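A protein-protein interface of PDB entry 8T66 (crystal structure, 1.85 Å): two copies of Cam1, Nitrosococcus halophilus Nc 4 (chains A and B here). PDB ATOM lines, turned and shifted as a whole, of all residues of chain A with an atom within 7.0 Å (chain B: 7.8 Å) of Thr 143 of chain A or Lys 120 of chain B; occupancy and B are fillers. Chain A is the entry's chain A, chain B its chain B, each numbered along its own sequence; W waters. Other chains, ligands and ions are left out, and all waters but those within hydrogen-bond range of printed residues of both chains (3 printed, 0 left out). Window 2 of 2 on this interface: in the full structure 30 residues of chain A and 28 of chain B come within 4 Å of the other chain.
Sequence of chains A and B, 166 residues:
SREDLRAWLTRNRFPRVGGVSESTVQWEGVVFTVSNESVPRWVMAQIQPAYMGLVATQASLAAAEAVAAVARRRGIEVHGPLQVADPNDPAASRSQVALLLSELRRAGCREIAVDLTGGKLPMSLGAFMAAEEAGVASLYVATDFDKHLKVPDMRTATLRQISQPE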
ATOM      1  N   VAL A  39      13.692   6.581 -13.104  1.00  0.00           N
ATOM      2  CA  VAL A  39      13.500   7.816 -12.346  1.00  0.00           C
ATOM      3  C   VAL A  39      12.005   8.112 -12.209  1.00  0.00           C
ATOM      4  O   VAL A  39      11.562   8.419 -11.100  1.00  0.00           O
ATOM      5  CB  VAL A  39      14.276   8.989 -12.970  1.00  0.00           C
ATOM      6  CG1 VAL A  39      14.005  10.256 -12.175  1.00  0.00           C
ATOM      7  CG2 VAL A  39      15.760   8.697 -12.955  1.00  0.00           C
ATOM      8  N   TRP A  42      10.576   6.009  -9.463  1.00  0.00           N
ATOM      9  CA  TRP A  42      10.903   6.513  -8.133  1.00  0.00           C
ATOM     10  C   TRP A  42       9.969   7.648  -7.726  1.00  0.00           C
ATOM     11  O   TRP A  42       9.472   7.678  -6.592  1.00  0.00           O
ATOM     12  CB  TRP A  42      12.360   6.986  -8.101  1.00  0.00           C
ATOM     13  CG  TRP A  42      12.775   7.464  -6.734  1.00  0.00           C
ATOM     14  CD1 TRP A  42      13.226   6.689  -5.695  1.00  0.00           C
ATOM     15  CD2 TRP A  42      12.757   8.813  -6.249  1.00  0.00           C
ATOM     16  NE1 TRP A  42      13.492   7.478  -4.598  1.00  0.00           N
ATOM     17  CE2 TRP A  42      13.212   8.782  -4.910  1.00  0.00           C
ATOM     18  CE3 TRP A  42      12.408  10.044  -6.817  1.00  0.00           C
ATOM     19  CZ2 TRP A  42      13.322   9.935  -4.128  1.00  0.00           C
ATOM     20  CZ3 TRP A  42      12.515  11.192  -6.035  1.00  0.00           C
ATOM     21  CH2 TRP A  42      12.978  11.128  -4.708  1.00  0.00           C
ATOM     22  N   LEU A 121      17.778  18.368 -22.896  1.00  0.00           N
ATOM     23  CA  LEU A 121      17.502  19.667 -22.286  1.00  0.00           C
ATOM     24  C   LEU A 121      16.342  20.413 -22.939  1.00  0.00           C
ATOM     25  O   LEU A 121      15.542  21.012 -22.196  1.00  0.00           O
ATOM     26  CB  LEU A 121      18.778  20.533 -22.288  1.00  0.00           C
ATOM     27  CG  LEU A 121      18.729  21.934 -21.657  1.00  0.00           C
ATOM     28  CD1 LEU A 121      20.101  22.337 -21.135  1.00  0.00           C
ATOM     29  CD2 LEU A 121      18.253  22.985 -22.684  1.00  0.00           C
ATOM     30  N   TYR A 140      12.476  18.362 -10.218  1.00  0.00           N
ATOM     31  CA  TYR A 140      13.687  17.755 -10.760  1.00  0.00           C
ATOM     32  C   TYR A 140      14.203  16.749  -9.744  1.00  0.00           C
ATOM     33  O   TYR A 140      14.280  17.064  -8.548  1.00  0.00           O
ATOM     34  CB  TYR A 140      14.761  18.821 -11.036  1.00  0.00           C
ATOM     35  CG  TYR A 140      16.107  18.247 -11.431  1.00  0.00           C
ATOM     36  CD1 TYR A 140      16.351  17.843 -12.740  1.00  0.00           C
ATOM     37  CD2 TYR A 140      17.136  18.118 -10.499  1.00  0.00           C
ATOM     38  CE1 TYR A 140      17.584  17.314 -13.115  1.00  0.00           C
ATOM     39  CE2 TYR A 140      18.375  17.593 -10.866  1.00  0.00           C
ATOM     40  CZ  TYR A 140      18.588  17.186 -12.171  1.00  0.00           C
ATOM     41  OH  TYR A 140      19.812  16.666 -12.521  1.00  0.00           O
ATOM     42  N   VAL A 141      14.565  15.553 -10.199  1.00  0.00           N
ATOM     43  CA  VAL A 141      15.096  14.535  -9.290  1.00  0.00           C
ATOM     44  C   VAL A 141      16.613  14.658  -9.287  1.00  0.00           C
ATOM     45  O   VAL A 141      17.278  14.321 -10.268  1.00  0.00           O
ATOM     46  CB  VAL A 141      14.659  13.117  -9.678  1.00  0.00           C
ATOM     47  CG1 VAL A 141      15.268  12.097  -8.701  1.00  0.00           C
ATOM     48  CG2 VAL A 141      13.144  13.023  -9.683  1.00  0.00           C
ATOM     49  N   ALA A 142      17.159  15.153  -8.186  1.00  0.00           N
ATOM     50  CA  ALA A 142      18.597  15.322  -8.053  1.00  0.00           C
ATOM     51  C   ALA A 142      19.192  14.047  -7.477  1.00  0.00           C
ATOM     52  O   ALA A 142      18.714  13.541  -6.453  1.00  0.00           O
ATOM     53  CB  ALA A 142      18.916  16.514  -7.146  1.00  0.00           C
ATOM     54  N   THR A 143      20.225  13.527  -8.139  1.00  0.00           N
ATOM     55  CA  THR A 143      20.944  12.358  -7.647  1.00  0.00           C
ATOM     56  C   THR A 143      22.440  12.561  -7.824  1.00  0.00           C
ATOM     57  O   THR A 143      22.890  13.349  -8.666  1.00  0.00           O
ATOM     58  CB  THR A 143      20.550  11.074  -8.387  1.00  0.00           C
ATOM     59  OG1 THR A 143      20.824  11.240  -9.788  1.00  0.00           O
ATOM     60  CG2 THR A 143      19.082  10.766  -8.193  1.00  0.00           C
ATOM     61  N   ASP A 144      23.209  11.818  -7.033  1.00  0.00           N
ATOM     62  CA  ASP A 144      24.601  11.571  -7.374  1.00  0.00           C
ATOM     63  C   ASP A 144      24.682  10.397  -8.340  1.00  0.00           C
ATOM     64  O   ASP A 144      23.778   9.563  -8.419  1.00  0.00           O
ATOM     65  CB  ASP A 144      25.429  11.268  -6.123  1.00  0.00           C
ATOM     66  CG  ASP A 144      25.493  12.439  -5.167  1.00  0.00           C
ATOM     67  OD1 ASP A 144      25.644  13.592  -5.629  1.00  0.00           O
ATOM     68  OD2 ASP A 144      25.392  12.208  -3.944  1.00  0.00           O
ATOM     69  N   PHE A 145      25.783  10.334  -9.084  1.00  0.00           N
ATOM     70  CA  PHE A 145      25.974   9.249 -10.036  1.00  0.00           C
ATOM     71  C   PHE A 145      26.537   8.017  -9.339  1.00  0.00           C
ATOM     72  O   PHE A 145      27.435   8.115  -8.494  1.00  0.00           O
ATOM     73  CB  PHE A 145      26.911   9.683 -11.156  1.00  0.00           C
ATOM     74  CG  PHE A 145      26.928   8.745 -12.338  1.00  0.00           C
ATOM     75  CD1 PHE A 145      25.852   8.686 -13.214  1.00  0.00           C
ATOM     76  CD2 PHE A 145      28.032   7.946 -12.586  1.00  0.00           C
ATOM     77  CE1 PHE A 145      25.879   7.845 -14.310  1.00  0.00           C
ATOM     78  CE2 PHE A 145      28.061   7.099 -13.680  1.00  0.00           C
ATOM     79  CZ  PHE A 145      26.986   7.058 -14.546  1.00  0.00           C
ATOM     80  N   ASP A 146      25.996   6.855  -9.689  1.00  0.00           N
ATOM     81  CA  ASP A 146      26.494   5.590  -9.157  1.00  0.00           C
ATOM     82  C   ASP A 146      27.763   5.218  -9.921  1.00  0.00           C
ATOM     83  O   ASP A 146      27.700   4.789 -11.079  1.00  0.00           O
ATOM     84  CB  ASP A 146      25.421   4.511  -9.267  1.00  0.00           C
ATOM     85  CG  ASP A 146      25.780   3.237  -8.518  1.00  0.00           C
ATOM     86  OD1 ASP A 146      26.980   2.979  -8.273  1.00  0.00           O
ATOM     87  OD2 ASP A 146      24.851   2.478  -8.179  1.00  0.00           O
ATOM     88  N   VAL A 151      24.827   4.499 -13.476  1.00  0.00           N
ATOM     89  CA  VAL A 151      23.474   5.044 -13.635  1.00  0.00           C
ATOM     90  C   VAL A 151      23.194   6.017 -12.491  1.00  0.00           C
ATOM     91  O   VAL A 151      23.977   6.071 -11.531  1.00  0.00           O
ATOM     92  CB  VAL A 151      22.410   3.931 -13.664  1.00  0.00           C
ATOM     93  CG1 VAL A 151      22.647   2.936 -14.806  1.00  0.00           C
ATOM     94  CG2 VAL A 151      22.351   3.228 -12.318  1.00  0.00           C
ATOM     95  N   PRO A 152      22.106   6.795 -12.534  1.00  0.00           N
ATOM     96  CA  PRO A 152      21.777   7.641 -11.380  1.00  0.00           C
ATOM     97  C   PRO A 152      21.584   6.800 -10.130  1.00  0.00           C
ATOM     98  O   PRO A 152      20.903   5.774 -10.150  1.00  0.00           O
ATOM     99  CB  PRO A 152      20.476   8.332 -11.801  1.00  0.00           C
ATOM    100  CG  PRO A 152      20.550   8.371 -13.298  1.00  0.00           C
ATOM    101  CD  PRO A 152      21.216   7.074 -13.680  1.00  0.00           C
ATOM    102  N   ASP A 153      22.197   7.245  -9.039  1.00  0.00           N
ATOM    103  CA  ASP A 153      22.077   6.556  -7.754  1.00  0.00           C
ATOM    104  C   ASP A 153      20.797   7.024  -7.077  1.00  0.00           C
ATOM    105  O   ASP A 153      20.758   8.093  -6.467  1.00  0.00           O
ATOM    106  CB  ASP A 153      23.301   6.828  -6.889  1.00  0.00           C
ATOM    107  CG  ASP A 153      23.359   5.928  -5.666  1.00  0.00           C
ATOM    108  OD1 ASP A 153      22.350   5.252  -5.374  1.00  0.00           O
ATOM    109  OD2 ASP A 153      24.412   5.904  -5.004  1.00  0.00           O
ATOM    110  N   MET A 154      19.749   6.203  -7.171  1.00  0.00           N
ATOM    111  CA  MET A 154      18.451   6.543  -6.602  1.00  0.00           C
ATOM    112  C   MET A 154      18.441   6.503  -5.073  1.00  0.00           C
ATOM    113  O   MET A 154      17.531   7.062  -4.455  1.00  0.00           O
ATOM    114  CB  MET A 154      17.389   5.609  -7.184  1.00  0.00           C
ATOM    115  CG  MET A 154      17.330   5.637  -8.709  1.00  0.00           C
ATOM    116  SD  MET A 154      17.238   7.304  -9.422  1.00  0.00           S
ATOM    117  CE  MET A 154      15.704   7.862  -8.711  1.00  0.00           C
ATOM    118  N   ARG A 155      19.442   5.883  -4.443  1.00  0.00           N
ATOM    119  CA  ARG A 155      19.598   6.031  -3.001  1.00  0.00           C
ATOM    120  C   ARG A 155      19.866   7.476  -2.603  1.00  0.00           C
ATOM    121  O   ARG A 155      19.650   7.841  -1.442  1.00  0.00           O
ATOM    122  CB  ARG A 155      20.743   5.144  -2.494  1.00  0.00           C
ATOM    123  CG  ARG A 155      20.551   3.664  -2.777  1.00  0.00           C
ATOM    124  CD  ARG A 155      21.844   2.886  -2.511  1.00  0.00           C
ATOM    125  NE  ARG A 155      22.914   3.311  -3.409  1.00  0.00           N
ATOM    126  CZ  ARG A 155      24.059   2.655  -3.573  1.00  0.00           C
ATOM    127  NH1 ARG A 155      24.287   1.537  -2.894  1.00  0.00           N
ATOM    128  NH2 ARG A 155      24.974   3.118  -4.416  1.00  0.00           N
ATOM    129  N   THR A 156      20.341   8.304  -3.527  1.00  0.00           N
ATOM    130  CA  THR A 156      20.632   9.696  -3.226  1.00  0.00           C
ATOM    131  C   THR A 156      19.543  10.644  -3.708  1.00  0.00           C
ATOM    132  O   THR A 156      19.670  11.861  -3.514  1.00  0.00           O
ATOM    133  CB  THR A 156      21.981  10.094  -3.831  1.00  0.00           C
ATOM    134  OG1 THR A 156      21.871  10.176  -5.261  1.00  0.00           O
ATOM    135  CG2 THR A 156      23.035   9.059  -3.473  1.00  0.00           C
ATOM    136  N   ALA A 157      18.462  10.113  -4.283  1.00  0.00           N
ATOM    137  CA  ALA A 157      17.476  10.942  -4.967  1.00  0.00           C
ATOM    138  C   ALA A 157      16.791  11.911  -4.012  1.00  0.00           C
ATOM    139  O   ALA A 157      16.336  11.534  -2.922  1.00  0.00           O
ATOM    140  CB  ALA A 157      16.429  10.067  -5.659  1.00  0.00           C
ATOM    141  N   THR A 158      16.717  13.164  -4.443  1.00  0.00           N
ATOM    142  CA  THR A 158      15.996  14.226  -3.757  1.00  0.00           C
ATOM    143  C   THR A 158      15.063  14.878  -4.766  1.00  0.00           C
ATOM    144  O   THR A 158      15.482  15.168  -5.887  1.00  0.00           O
ATOM    145  CB  THR A 158      16.976  15.260  -3.181  1.00  0.00           C
ATOM    146  OG1 THR A 158      17.897  14.598  -2.307  1.00  0.00           O
ATOM    147  CG2 THR A 158      16.223  16.333  -2.391  1.00  0.00           C
ATOM    148  N   THR B  33      26.666  28.483 -18.603  1.00  0.00           N
ATOM    149  CA  THR B  33      26.803  27.579 -17.462  1.00  0.00           C
ATOM    150  C   THR B  33      27.800  26.504 -17.874  1.00  0.00           C
ATOM    151  O   THR B  33      27.729  26.002 -18.996  1.00  0.00           O
ATOM    152  CB  THR B  33      25.445  26.956 -17.103  1.00  0.00           C
ATOM    153  OG1 THR B  33      24.744  26.627 -18.320  1.00  0.00           O
ATOM    154  CG2 THR B  33      24.608  27.946 -16.310  1.00  0.00           C
ATOM    155  N   VAL B  34      28.758  26.171 -17.016  1.00  0.00           N
ATOM    156  CA  VAL B  34      29.919  25.415 -17.472  1.00  0.00           C
ATOM    157  C   VAL B  34      29.969  24.044 -16.820  1.00  0.00           C
ATOM    158  O   VAL B  34      29.898  23.924 -15.591  1.00  0.00           O
ATOM    159  CB  VAL B  34      31.231  26.172 -17.217  1.00  0.00           C
ATOM    160  CG1 VAL B  34      32.421  25.310 -17.646  1.00  0.00           C
ATOM    161  CG2 VAL B  34      31.203  27.511 -17.967  1.00  0.00           C
ATOM    162  N   SER B  35      30.119  23.017 -17.650  1.00  0.00           N
ATOM    163  CA  SER B  35      30.533  21.696 -17.208  1.00  0.00           C
ATOM    164  C   SER B  35      31.814  21.256 -17.902  1.00  0.00           C
ATOM    165  O   SER B  35      32.751  20.820 -17.231  1.00  0.00           O
ATOM    166  CB  SER B  35      29.406  20.677 -17.448  1.00  0.00           C
ATOM    167  OG  SER B  35      28.822  20.893 -18.728  1.00  0.00           O
ATOM    168  N   THR B  57      30.759  25.388 -11.081  1.00  0.00           N
ATOM    169  CA  THR B  57      30.795  24.812  -9.744  1.00  0.00           C
ATOM    170  C   THR B  57      32.247  24.642  -9.311  1.00  0.00           C
ATOM    171  O   THR B  57      33.170  24.871 -10.080  1.00  0.00           O
ATOM    172  CB  THR B  57      30.088  23.455  -9.713  1.00  0.00           C
ATOM    173  OG1 THR B  57      30.827  22.534 -10.523  1.00  0.00           O
ATOM    174  CG2 THR B  57      28.675  23.579 -10.253  1.00  0.00           C
ATOM    175  N   SER B  60      33.544  22.172 -11.840  1.00  0.00           N
ATOM    176  CA  SER B  60      33.786  22.585 -13.217  1.00  0.00           C
ATOM    177  C   SER B  60      34.608  23.868 -13.316  1.00  0.00           C
ATOM    178  O   SER B  60      34.812  24.373 -14.424  1.00  0.00           O
ATOM    179  CB  SER B  60      32.445  22.743 -13.968  1.00  0.00           C
ATOM    180  OG  SER B  60      31.698  23.834 -13.472  1.00  0.00           O
ATOM    181  N   ASP B  86      26.119  24.420  -5.313  1.00  0.00           N
ATOM    182  CA  ASP B  86      25.394  23.168  -5.535  1.00  0.00           C
ATOM    183  C   ASP B  86      24.847  23.102  -6.956  1.00  0.00           C
ATOM    184  O   ASP B  86      23.954  23.884  -7.300  1.00  0.00           O
ATOM    185  CB  ASP B  86      24.265  23.055  -4.504  1.00  0.00           C
ATOM    186  CG  ASP B  86      23.451  21.776  -4.636  1.00  0.00           C
ATOM    187  OD1 ASP B  86      23.824  20.876  -5.412  1.00  0.00           O
ATOM    188  OD2 ASP B  86      22.433  21.669  -3.921  1.00  0.00           O
ATOM    189  N   PRO B  87      25.331  22.180  -7.802  1.00  0.00           N
ATOM    190  CA  PRO B  87      24.806  22.089  -9.177  1.00  0.00           C
ATOM    191  C   PRO B  87      23.361  21.630  -9.242  1.00  0.00           C
ATOM    192  O   PRO B  87      22.752  21.709 -10.315  1.00  0.00           O
ATOM    193  CB  PRO B  87      25.732  21.059  -9.836  1.00  0.00           C
ATOM    194  CG  PRO B  87      26.132  20.169  -8.672  1.00  0.00           C
ATOM    195  CD  PRO B  87      26.296  21.105  -7.510  1.00  0.00           C
ATOM    196  N   ASN B  88      22.793  21.132  -8.147  1.00  0.00           N
ATOM    197  CA  ASN B  88      21.417  20.665  -8.169  1.00  0.00           C
ATOM    198  C   ASN B  88      20.417  21.759  -7.831  1.00  0.00           C
ATOM    199  O   ASN B  88      19.217  21.500  -7.860  1.00  0.00           O
ATOM    200  CB  ASN B  88      21.239  19.489  -7.195  1.00  0.00           C
ATOM    201  CG  ASN B  88      22.003  18.257  -7.637  1.00  0.00           C
ATOM    202  OD1 ASN B  88      21.924  17.840  -8.800  1.00  0.00           O
ATOM    203  ND2 ASN B  88      22.764  17.679  -6.720  1.00  0.00           N
ATOM    204  N   ASP B  89      20.871  22.956  -7.476  1.00  0.00           N
ATOM    205  CA  ASP B  89      19.955  23.993  -7.035  1.00  0.00           C
ATOM    206  C   ASP B  89      19.881  25.080  -8.084  1.00  0.00           C
ATOM    207  O   ASP B  89      20.919  25.644  -8.458  1.00  0.00           O
ATOM    208  CB  ASP B  89      20.402  24.601  -5.690  1.00  0.00           C
ATOM    209  CG  ASP B  89      19.586  25.840  -5.284  1.00  0.00           C
ATOM    210  OD1 ASP B  89      18.327  25.789  -5.249  1.00  0.00           O
ATOM    211  OD2 ASP B  89      20.237  26.883  -4.986  1.00  0.00           O
ATOM    212  N   SER B  93      22.438  29.473  -9.466  1.00  0.00           N
ATOM    213  CA  SER B  93      22.767  29.738 -10.863  1.00  0.00           C
ATOM    214  C   SER B  93      21.972  30.908 -11.396  1.00  0.00           C
ATOM    215  O   SER B  93      22.501  31.740 -12.150  1.00  0.00           O
ATOM    216  CB  SER B  93      22.526  28.488 -11.691  1.00  0.00           C
ATOM    217  OG  SER B  93      23.591  27.575 -11.455  1.00  0.00           O
ATOM    218  N   LEU B 116      22.661  27.569 -22.520  1.00  0.00           N
ATOM    219  CA  LEU B 116      22.157  26.711 -21.441  1.00  0.00           C
ATOM    220  C   LEU B 116      22.790  25.333 -21.421  1.00  0.00           C
ATOM    221  O   LEU B 116      22.527  24.567 -20.481  1.00  0.00           O
ATOM    222  CB  LEU B 116      20.638  26.512 -21.588  1.00  0.00           C
ATOM    223  CG  LEU B 116      19.750  27.738 -21.525  1.00  0.00           C
ATOM    224  CD1 LEU B 116      18.313  27.317 -21.431  1.00  0.00           C
ATOM    225  CD2 LEU B 116      20.143  28.547 -20.309  1.00  0.00           C
ATOM    226  N   THR B 117      23.585  24.996 -22.443  1.00  0.00           N
ATOM    227  CA  THR B 117      23.947  23.604 -22.697  1.00  0.00           C
ATOM    228  C   THR B 117      24.712  23.001 -21.522  1.00  0.00           C
ATOM    229  O   THR B 117      24.407  21.887 -21.068  1.00  0.00           O
ATOM    230  CB  THR B 117      24.784  23.507 -23.972  1.00  0.00           C
ATOM    231  OG1 THR B 117      24.181  24.298 -25.009  1.00  0.00           O
ATOM    232  CG2 THR B 117      24.899  22.053 -24.416  1.00  0.00           C
ATOM    233  N   GLY B 118      25.708  23.725 -21.017  1.00  0.00           N
ATOM    234  CA  GLY B 118      26.599  23.178 -20.014  1.00  0.00           C
ATOM    235  C   GLY B 118      25.992  23.169 -18.627  1.00  0.00           C
ATOM    236  O   GLY B 118      24.967  23.804 -18.369  1.00  0.00           O
ATOM    237  N   GLY B 119      26.662  22.432 -17.732  1.00  0.00           N
ATOM    238  CA  GLY B 119      26.255  22.316 -16.344  1.00  0.00           C
ATOM    239  C   GLY B 119      25.109  21.336 -16.168  1.00  0.00           C
ATOM    240  O   GLY B 119      24.520  20.842 -17.127  1.00  0.00           O
ATOM    241  N   LYS B 120      24.791  21.052 -14.902  1.00  0.00           N
ATOM    242  CA  LYS B 120      23.664  20.199 -14.558  1.00  0.00           C
ATOM    243  C   LYS B 120      22.352  20.903 -14.891  1.00  0.00           C
ATOM    244  O   LYS B 120      22.293  22.126 -15.008  1.00  0.00           O
ATOM    245  CB  LYS B 120      23.720  19.817 -13.072  1.00  0.00           C
ATOM    246  CG  LYS B 120      23.161  18.441 -12.797  1.00  0.00           C
ATOM    247  CD  LYS B 120      23.755  17.803 -11.549  1.00  0.00           C
ATOM    248  CE  LYS B 120      23.351  16.341 -11.477  1.00  0.00           C
ATOM    249  NZ  LYS B 120      23.329  15.878 -10.071  1.00  0.00           N
ATOM    250  N   LEU B 121      21.295  20.118 -15.096  1.00  0.00           N
ATOM    251  CA  LEU B 121      20.039  20.728 -15.543  1.00  0.00           C
ATOM    252  C   LEU B 121      19.546  21.844 -14.626  1.00  0.00           C
ATOM    253  O   LEU B 121      19.121  22.890 -15.152  1.00  0.00           O
ATOM    254  CB  LEU B 121      18.946  19.663 -15.726  1.00  0.00           C
ATOM    255  CG  LEU B 121      17.612  20.202 -16.281  1.00  0.00           C
ATOM    256  CD1 LEU B 121      17.806  20.930 -17.626  1.00  0.00           C
ATOM    257  CD2 LEU B 121      16.545  19.102 -16.409  1.00  0.00           C
ATOM    258  N   PRO B 122      19.598  21.733 -13.293  1.00  0.00           N
ATOM    259  CA  PRO B 122      19.152  22.876 -12.482  1.00  0.00           C
ATOM    260  C   PRO B 122      19.980  24.111 -12.725  1.00  0.00           C
ATOM    261  O   PRO B 122      19.450  25.221 -12.621  1.00  0.00           O
ATOM    262  CB  PRO B 122      19.301  22.380 -11.026  1.00  0.00           C
ATOM    263  CG  PRO B 122      19.220  20.895 -11.138  1.00  0.00           C
ATOM    264  CD  PRO B 122      19.948  20.581 -12.441  1.00  0.00           C
ATOM    265  N   MET B 123      21.271  23.958 -13.013  1.00  0.00           N
ATOM    266  CA  MET B 123      22.073  25.128 -13.351  1.00  0.00           C
ATOM    267  C   MET B 123      21.541  25.773 -14.624  1.00  0.00           C
ATOM    268  O   MET B 123      21.377  26.998 -14.702  1.00  0.00           O
ATOM    269  CB  MET B 123      23.545  24.738 -13.520  1.00  0.00           C
ATOM    270  CG  MET B 123      24.267  24.323 -12.228  1.00  0.00           C
ATOM    271  SD  MET B 123      25.844  23.525 -12.610  1.00  0.00           S
ATOM    272  CE  MET B 123      26.759  24.853 -13.424  1.00  0.00           C
ATOM    273  N   SER B 124      21.251  24.959 -15.630  1.00  0.00           N
ATOM    274  CA  SER B 124      20.683  25.486 -16.867  1.00  0.00           C
ATOM    275  C   SER B 124      19.318  26.126 -16.630  1.00  0.00           C
ATOM    276  O   SER B 124      19.010  27.173 -17.205  1.00  0.00           O
ATOM    277  CB  SER B 124      20.566  24.359 -17.887  1.00  0.00           C
ATOM    278  OG  SER B 124      21.838  23.848 -18.175  1.00  0.00           O
ATOM    279  N   LEU B 125      18.487  25.522 -15.766  1.00  0.00           N
ATOM    280  CA  LEU B 125      17.176  26.111 -15.530  1.00  0.00           C
ATOM    281  C   LEU B 125      17.294  27.434 -14.783  1.00  0.00           C
ATOM    282  O   LEU B 125      16.552  28.376 -15.075  1.00  0.00           O
ATOM    283  CB  LEU B 125      16.283  25.138 -14.777  1.00  0.00           C
ATOM    284  CG  LEU B 125      15.673  24.020 -15.628  1.00  0.00           C
ATOM    285  CD1 LEU B 125      15.208  22.906 -14.710  1.00  0.00           C
ATOM    286  CD2 LEU B 125      14.499  24.571 -16.432  1.00  0.00           C
ATOM    287  N   GLY B 126      18.209  27.532 -13.816  1.00  0.00           N
ATOM    288  CA  GLY B 126      18.437  28.830 -13.179  1.00  0.00           C
ATOM    289  C   GLY B 126      18.928  29.877 -14.168  1.00  0.00           C
ATOM    290  O   GLY B 126      18.494  31.031 -14.132  1.00  0.00           O
ATOM    291  N   ALA B 127      19.809  29.476 -15.082  1.00  0.00           N
ATOM    292  CA  ALA B 127      20.307  30.393 -16.106  1.00  0.00           C
ATOM    293  C   ALA B 127      19.184  30.840 -17.025  1.00  0.00           C
ATOM    294  O   ALA B 127      19.116  32.015 -17.412  1.00  0.00           O
ATOM    295  CB  ALA B 127      21.411  29.724 -16.929  1.00  0.00           C
HETATM  296  O   HOH W   1      20.930  16.800 -14.919  1.00  0.00           O
HETATM  297  O   HOH W   2      20.691  14.640 -10.895  1.00  0.00           O
HETATM  298  O   HOH W   3      24.764  13.332 -11.463  1.00  0.00           O
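Printed residues of chain B within 4 Å of Leu 121 of chain A: Leu 116 and Ser 124.
Of chain B, only Asn 88 comes within 4 Å of Ala 142 of chain A.
Thr 143 of chain A touches just one residue of chain B: Lys 120 (2.9 Å).
Pro 152 of chain A touches none of the printed residues of chain B.
Arg 155 of chain A touches none of the printed residues of chain B.
Printed residues of chain A within 4 Å of Leu 116 of chain B: Leu 121 (3.4 Å).
Lys 120 of chain B touches just these residues of chain A: Tyr 140 and Thr 143.
Of the printed residues of chain A, Ser 124 of chain B touches Leu 121.
The nearest printed residue of chain B that does not touch Leu 121 of chain A is Leu 121 of chain B (4.3 Å).
Position printed for both chains: 121.
Of the 7 pairs that touch across the chains among the printed residues, none has its exchanged pair printed and touching as well.
The side-chain amino group (NZ) of Lys 120 of chain B is in hydrogen-bond range of the backbone carbonyl oxygen (O) of Thr 143 of chain A (2.9 Å).
Printed residues of chain B that touch a printed residue of chain A: Asn 88, Leu 116, Lys 120, Leu 121, Pro 122 and Ser 124.
Hydrophobic or aromatic side chains of chain B within 4 Å of the printed part of chain A: Leu 121 and Pro 122.
Of the 18 printed residues of chain A, 4 touch a printed residue of chain B.
Printed residues of chain A that touch a printed residue of chain B: Leu 121, Tyr 140, Ala 142 and Thr 143.
Hydrophobic or aromatic side chains of chain A within 4 Å of the printed part of chain B: Leu 121, Tyr 140 and Ala 142.
Among the printed residues, 7 pairs touch across the chains.
Among the printed residues, no Asp or Glu carboxylate lies within 4 Å of a Lys or Arg side-chain nitrogen of the other chain.
Water W1 lies within hydrogen-bond range of the side-chain hydroxyl (OH) of Tyr 140 of chain A and the backbone NH (N) of Leu 121 of chain B.
Water W2 lies within hydrogen-bond range of the side-chain hydroxyl of Tyr 140 of chain A (2.7 Å), the backbone NH of Thr 143 of chain A (3.0 Å), the side-chain amino group of Lys 120 of chain B (3.0 Å) and the backbone carbonyl oxygen of Val 141 of chain A (3.5 Å).
Water W3 lies within hydrogen-bond range of the side-chain amino group (NZ) of Lys 120 of chain B and the backbone carbonyl oxygen (O) of Thr 143 of chain A.
The backbone carbonyl oxygen (O) of Leu 116 of chain B sits at hydrogen-bond distance from the side-chain hydroxyl (OG) of Ser 124 of chain B (2.5 Å).
The backbone NH (N) of Asn 88 of chain B sits at hydrogen-bond distance from the side-chain carboxylate (OD1) of Asp 86 of chain B, 2.9 Å away.
The backbone carbonyl oxygen (O) of Gly 118 of chain B is in hydrogen-bond range of the side-chain hydroxyl (OG) of Ser 124 of chain B (3.1 Å).
OD1 of Asn 88 of chain B lies within hydrogen-bond range of NZ of Lys 120 of chain B.
SD of Met 123 of chain B is in hydrogen-bond range of N of Lys 120 of chain B (3.5 Å).
O of Thr 158 of chain A is in hydrogen-bond range of N of Ala 142 of chain A, 2.8 Å away.
Among the printed residues, pairs that only touch across the chains: Leu 121 of chain A with Leu 116 of chain B (3.4 Å), Leu 121 of chain A with Ser 124 of chain B (3.7 Å), Tyr 140 of chain A with Lys 120 of chain B (3.7 Å), Tyr 140 of chain A with Leu 121 of chain B (3.8 Å), Tyr 140 of chain A with Pro 122 of chain B (3.4 Å) and Ala 142 of chain A with Asn 88 of chain B (3.6 Å).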
